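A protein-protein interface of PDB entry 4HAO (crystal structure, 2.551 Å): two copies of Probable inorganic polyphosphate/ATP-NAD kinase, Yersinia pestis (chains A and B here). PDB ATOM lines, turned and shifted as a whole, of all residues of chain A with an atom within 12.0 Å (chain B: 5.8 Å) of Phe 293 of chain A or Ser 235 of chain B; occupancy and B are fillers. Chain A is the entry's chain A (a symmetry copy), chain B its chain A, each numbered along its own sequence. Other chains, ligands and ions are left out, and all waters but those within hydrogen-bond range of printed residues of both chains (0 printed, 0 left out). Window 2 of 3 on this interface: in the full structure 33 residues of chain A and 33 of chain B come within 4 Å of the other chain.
The backbone carbonyl oxygen (O) of Ser 289 of chain A lies within hydrogen-bond range of the backbone NH (N) of Ser 174 of chain B (3.0 Å). O of Lys 290 of chain A is in hydrogen-bond range of OG of Ser 174 of chain B (2.5 Å). The side-chain carboxylate of Glu 164 of chain B is in hydrogen-bond range of the backbone NH of Phe 293 of chain A, at 2.9 Å. The backbone NH (N) of Leu 292 of chain A is in hydrogen-bond range of the side-chain hydroxyl (OG) of Ser 174 of chain B (3.2 Å). The side-chain carboxylate (OE2) of Glu 164 of chain B sits at hydrogen-bond distance from the backbone NH (N) of Leu 292 of chain A.
The backbone carbonyl oxygen (O) of Lys 233 of chain B is in hydrogen-bond range of the backbone NH (N) of Glu 164 of chain B.
Glu 164 of chain B touches Lys 291 of chain A. Lys 291 of chain A touches Ser 174 of chain B (CA to OG, 3.6 Å). Glu 162 of chain B touches Leu 292 of chain A (OE1 to CD1, 3.5 Å). Phe 293 of chain A touches Lys 233 of chain B. C of Phe 234 of chain B touches CE2 of Phe 293 of chain A, at 3.6 Å. Phe 293 of chain A touches Ser 235 of chain B (CE1 to CB, 3.3 Å).
Of the printed residues of chain B, Lys 290 of chain A touches Ser 174. Of the printed residues of chain B, Leu 292 of chain A touches Glu 162 (3.5 Å), Glu 164 (2.8 Å) and Ser 174 (3.2 Å). Phe 293 of chain A touches four residues of chain B. Of the printed residues of chain A, Glu 162 of chain B touches Leu 292 (3.5 Å). Glu 164 of chain B touches just these residues of chain A: Lys 291 (3.3 Å), Leu 292 (2.8 Å) and Phe 293 (2.9 Å). Printed residues of chain A within 4 Å of Ser 174 of chain B: Ser 289, Lys 290, Lys 291 and Leu 292. Lys 233 of chain B touches just one residue of chain A: Phe 293 (3.8 Å). Phe 234 of chain B touches one residue of chain A. Ser 235 of chain B touches just one residue of chain A: Phe 293. No residue of chain A comes within 4 Å of Ile 237 of chain B. Glu 255 of chain B touches none of the printed residues of chain A. The nearest residue of chain A that does not touch Ser 235 of chain B is Leu 292 of chain A (6.5 Å).
Of the 5 printed residues of chain A, 5 touch a printed residue of chain B. Printed residues of chain A that touch a printed residue of chain B: Ser 289, Lys 290, Lys 291, Leu 292 and Phe 293. Of the 10 printed residues of chain B, 6 touch a printed residue of chain A. Among the printed residues, no Asp or Glu carboxylate lies within 4 Å of a Lys or Arg side-chain nitrogen of the other chain.
No position is printed for both chains.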
ATOM      1  N   SER A 289      24.557 -19.491  11.745  1.00  0.00           N
ATOM      2  CA  SER A 289      25.098 -18.667  10.671  1.00  0.00           C
ATOM      3  C   SER A 289      26.568 -18.359  10.857  1.00  0.00           C
ATOM      4  O   SER A 289      27.032 -18.062  11.968  1.00  0.00           O
ATOM      5  CB  SER A 289      24.334 -17.357  10.559  1.00  0.00           C
ATOM      6  OG  SER A 289      23.144 -17.548   9.836  1.00  0.00           O
ATOM      7  N   LYS A 290      27.294 -18.431   9.750  1.00  0.00           N
ATOM      8  CA  LYS A 290      28.695 -18.067   9.733  1.00  0.00           C
ATOM      9  C   LYS A 290      28.770 -16.589   9.461  1.00  0.00           C
ATOM     10  O   LYS A 290      27.742 -15.916   9.420  1.00  0.00           O
ATOM     11  CB  LYS A 290      29.443 -18.855   8.661  1.00  0.00           C
ATOM     12  CG  LYS A 290      29.639 -20.334   9.014  1.00  0.00           C
ATOM     13  CD  LYS A 290      30.378 -20.495  10.348  1.00  0.00           C
ATOM     14  CE  LYS A 290      30.436 -21.954  10.810  1.00  0.00           C
ATOM     15  NZ  LYS A 290      31.253 -22.828   9.925  1.00  0.00           N
ATOM     16  N   LYS A 291      29.983 -16.089   9.272  1.00  0.00           N
ATOM     17  CA  LYS A 291      30.210 -14.666   9.052  1.00  0.00           C
ATOM     18  C   LYS A 291      29.287 -14.097   7.967  1.00  0.00           C
ATOM     19  O   LYS A 291      29.190 -14.649   6.872  1.00  0.00           O
ATOM     20  CB  LYS A 291      31.683 -14.422   8.711  1.00  0.00           C
ATOM     21  CG  LYS A 291      32.123 -12.981   8.860  1.00  0.00           C
ATOM     22  CD  LYS A 291      33.635 -12.887   8.969  1.00  0.00           C
ATOM     23  CE  LYS A 291      34.141 -13.378  10.320  1.00  0.00           C
ATOM     24  NZ  LYS A 291      35.343 -12.598  10.777  1.00  0.00           N
ATOM     25  N   LEU A 292      28.593 -13.008   8.293  1.00  0.00           N
ATOM     26  CA  LEU A 292      27.647 -12.397   7.357  1.00  0.00           C
ATOM     27  C   LEU A 292      28.226 -11.271   6.493  1.00  0.00           C
ATOM     28  O   LEU A 292      27.724 -11.022   5.399  1.00  0.00           O
ATOM     29  CB  LEU A 292      26.387 -11.904   8.074  1.00  0.00           C
ATOM     30  CG  LEU A 292      25.367 -12.958   8.519  1.00  0.00           C
ATOM     31  CD1 LEU A 292      23.948 -12.397   8.457  1.00  0.00           C
ATOM     32  CD2 LEU A 292      25.502 -14.263   7.721  1.00  0.00           C
ATOM     33  N   PHE A 293      29.254 -10.580   6.976  1.00  0.00           N
ATOM     34  CA  PHE A 293      29.882  -9.528   6.174  1.00  0.00           C
ATOM     35  C   PHE A 293      31.400  -9.624   6.207  1.00  0.00           C
ATOM     36  O   PHE A 293      31.963 -10.356   7.017  1.00  0.00           O
ATOM     37  CB  PHE A 293      29.429  -8.119   6.593  1.00  0.00           C
ATOM     38  CG  PHE A 293      28.470  -8.091   7.757  1.00  0.00           C
ATOM     39  CD1 PHE A 293      27.125  -8.390   7.579  1.00  0.00           C
ATOM     40  CD2 PHE A 293      28.905  -7.735   9.025  1.00  0.00           C
ATOM     41  CE1 PHE A 293      26.239  -8.367   8.653  1.00  0.00           C
ATOM     42  CE2 PHE A 293      28.025  -7.702  10.099  1.00  0.00           C
ATOM     43  CZ  PHE A 293      26.690  -8.014   9.911  1.00  0.00           C
ATOM     44  N   GLU B 162      20.345  -7.843  11.542  1.00  0.00           N
ATOM     45  CA  GLU B 162      21.473  -8.760  11.350  1.00  0.00           C
ATOM     46  C   GLU B 162      22.686  -8.245  12.103  1.00  0.00           C
ATOM     47  O   GLU B 162      22.937  -7.047  12.136  1.00  0.00           O
ATOM     48  CB  GLU B 162      21.856  -8.880   9.879  1.00  0.00           C
ATOM     49  CG  GLU B 162      20.863  -9.595   8.995  1.00  0.00           C
ATOM     50  CD  GLU B 162      21.476  -9.997   7.662  1.00  0.00           C
ATOM     51  OE1 GLU B 162      21.039 -11.019   7.087  1.00  0.00           O
ATOM     52  OE2 GLU B 162      22.405  -9.296   7.198  1.00  0.00           O
ATOM     53  N   PHE B 163      23.445  -9.146  12.706  1.00  0.00           N
ATOM     54  CA  PHE B 163      24.652  -8.749  13.409  1.00  0.00           C
ATOM     55  C   PHE B 163      25.556  -9.948  13.644  1.00  0.00           C
ATOM     56  O   PHE B 163      25.140 -11.099  13.515  1.00  0.00           O
ATOM     57  CB  PHE B 163      24.311  -8.058  14.734  1.00  0.00           C
ATOM     58  CG  PHE B 163      23.508  -8.914  15.677  1.00  0.00           C
ATOM     59  CD1 PHE B 163      24.122  -9.570  16.726  1.00  0.00           C
ATOM     60  CD2 PHE B 163      22.137  -9.064  15.507  1.00  0.00           C
ATOM     61  CE1 PHE B 163      23.379 -10.352  17.584  1.00  0.00           C
ATOM     62  CE2 PHE B 163      21.391  -9.849  16.366  1.00  0.00           C
ATOM     63  CZ  PHE B 163      22.006 -10.490  17.403  1.00  0.00           C
ATOM     64  N   GLU B 164      26.809  -9.666  13.965  1.00  0.00           N
ATOM     65  CA  GLU B 164      27.760 -10.709  14.288  1.00  0.00           C
ATOM     66  C   GLU B 164      28.199 -10.499  15.715  1.00  0.00           C
ATOM     67  O   GLU B 164      28.253  -9.353  16.204  1.00  0.00           O
ATOM     68  CB  GLU B 164      28.957 -10.654  13.352  1.00  0.00           C
ATOM     69  CG  GLU B 164      28.601 -10.892  11.920  1.00  0.00           C
ATOM     70  CD  GLU B 164      29.769 -10.660  11.024  1.00  0.00           C
ATOM     71  OE1 GLU B 164      30.811 -10.184  11.531  1.00  0.00           O
ATOM     72  OE2 GLU B 164      29.650 -10.952   9.816  1.00  0.00           O
ATOM     73  N   SER B 174      27.000 -15.508  13.620  1.00  0.00           N
ATOM     74  CA  SER B 174      26.110 -14.484  13.088  1.00  0.00           C
ATOM     75  C   SER B 174      24.725 -14.671  13.669  1.00  0.00           C
ATOM     76  O   SER B 174      24.464 -15.664  14.350  1.00  0.00           O
ATOM     77  CB  SER B 174      26.009 -14.582  11.574  1.00  0.00           C
ATOM     78  OG  SER B 174      27.152 -14.047  10.941  1.00  0.00           O
ATOM     79  N   LYS B 233      28.890  -6.443  15.912  1.00  0.00           N
ATOM     80  CA  LYS B 233      29.204  -5.754  14.668  1.00  0.00           C
ATOM     81  C   LYS B 233      27.995  -5.810  13.759  1.00  0.00           C
ATOM     82  O   LYS B 233      27.283  -6.820  13.730  1.00  0.00           O
ATOM     83  CB  LYS B 233      30.417  -6.367  13.958  1.00  0.00           C
ATOM     84  CG  LYS B 233      31.751  -6.110  14.613  1.00  0.00           C
ATOM     85  CD  LYS B 233      32.887  -6.619  13.730  1.00  0.00           C
ATOM     86  CE  LYS B 233      34.258  -6.409  14.374  1.00  0.00           C
ATOM     87  NZ  LYS B 233      35.380  -6.952  13.551  1.00  0.00           N
ATOM     88  N   PHE B 234      27.770  -4.725  13.018  1.00  0.00           N
ATOM     89  CA  PHE B 234      26.568  -4.598  12.204  1.00  0.00           C
ATOM     90  C   PHE B 234      26.896  -4.306  10.747  1.00  0.00           C
ATOM     91  O   PHE B 234      27.942  -3.735  10.450  1.00  0.00           O
ATOM     92  CB  PHE B 234      25.681  -3.517  12.792  1.00  0.00           C
ATOM     93  CG  PHE B 234      25.486  -3.649  14.265  1.00  0.00           C
ATOM     94  CD1 PHE B 234      24.560  -4.543  14.769  1.00  0.00           C
ATOM     95  CD2 PHE B 234      26.241  -2.903  15.148  1.00  0.00           C
ATOM     96  CE1 PHE B 234      24.382  -4.686  16.136  1.00  0.00           C
ATOM     97  CE2 PHE B 234      26.065  -3.028  16.506  1.00  0.00           C
ATOM     98  CZ  PHE B 234      25.137  -3.925  17.004  1.00  0.00           C
ATOM     99  N   SER B 235      26.016  -4.716   9.841  1.00  0.00           N
ATOM    100  CA  SER B 235      26.248  -4.507   8.413  1.00  0.00           C
ATOM    101  C   SER B 235      26.034  -3.071   7.951  1.00  0.00           C
ATOM    102  O   SER B 235      26.966  -2.390   7.514  1.00  0.00           O
ATOM    103  CB  SER B 235      25.347  -5.404   7.567  1.00  0.00           C
ATOM    104  OG  SER B 235      25.407  -4.994   6.198  1.00  0.00           O
ATOM    105  N   HIS B 236      24.783  -2.635   8.017  1.00  0.00           N
ATOM    106  CA  HIS B 236      24.402  -1.325   7.520  1.00  0.00           C
ATOM    107  C   HIS B 236      23.291  -0.772   8.373  1.00  0.00           C
ATOM    108  O   HIS B 236      22.646  -1.501   9.118  1.00  0.00           O
ATOM    109  CB  HIS B 236      23.945  -1.408   6.069  1.00  0.00           C
ATOM    110  CG  HIS B 236      25.025  -1.089   5.081  1.00  0.00           C
ATOM    111  ND1 HIS B 236      25.462   0.195   4.853  1.00  0.00           N
ATOM    112  CD2 HIS B 236      25.747  -1.888   4.259  1.00  0.00           C
ATOM    113  CE1 HIS B 236      26.415   0.179   3.932  1.00  0.00           C
ATOM    114  NE2 HIS B 236      26.603  -1.071   3.556  1.00  0.00           N
ATOM    115  N   ILE B 237      23.070   0.528   8.280  1.00  0.00           N
ATOM    116  CA  ILE B 237      22.042   1.147   9.093  1.00  0.00           C
ATOM    117  C   ILE B 237      21.096   1.990   8.248  1.00  0.00           C
ATOM    118  O   ILE B 237      21.443   3.077   7.788  1.00  0.00           O
ATOM    119  CB  ILE B 237      22.665   2.013  10.204  1.00  0.00           C
ATOM    120  CG1 ILE B 237      23.742   1.216  10.940  1.00  0.00           C
ATOM    121  CG2 ILE B 237      21.608   2.469  11.188  1.00  0.00           C
ATOM    122  CD1 ILE B 237      23.189   0.190  11.862  1.00  0.00           C
ATOM    123  N   GLU B 255      26.071   4.257  12.258  1.00  0.00           N
ATOM    124  CA  GLU B 255      26.661   3.409  11.226  1.00  0.00           C
ATOM    125  C   GLU B 255      28.186   3.400  11.274  1.00  0.00           C
ATOM    126  O   GLU B 255      28.826   4.456  11.249  1.00  0.00           O
ATOM    127  CB  GLU B 255      26.185   3.853   9.842  1.00  0.00           C
ATOM    128  CG  GLU B 255      26.827   3.093   8.702  1.00  0.00           C
ATOM    129  CD  GLU B 255      25.834   2.738   7.617  1.00  0.00           C
ATOM    130  OE1 GLU B 255      24.959   3.580   7.313  1.00  0.00           O
ATOM    131  OE2 GLU B 255      25.924   1.610   7.083  1.00  0.00           O
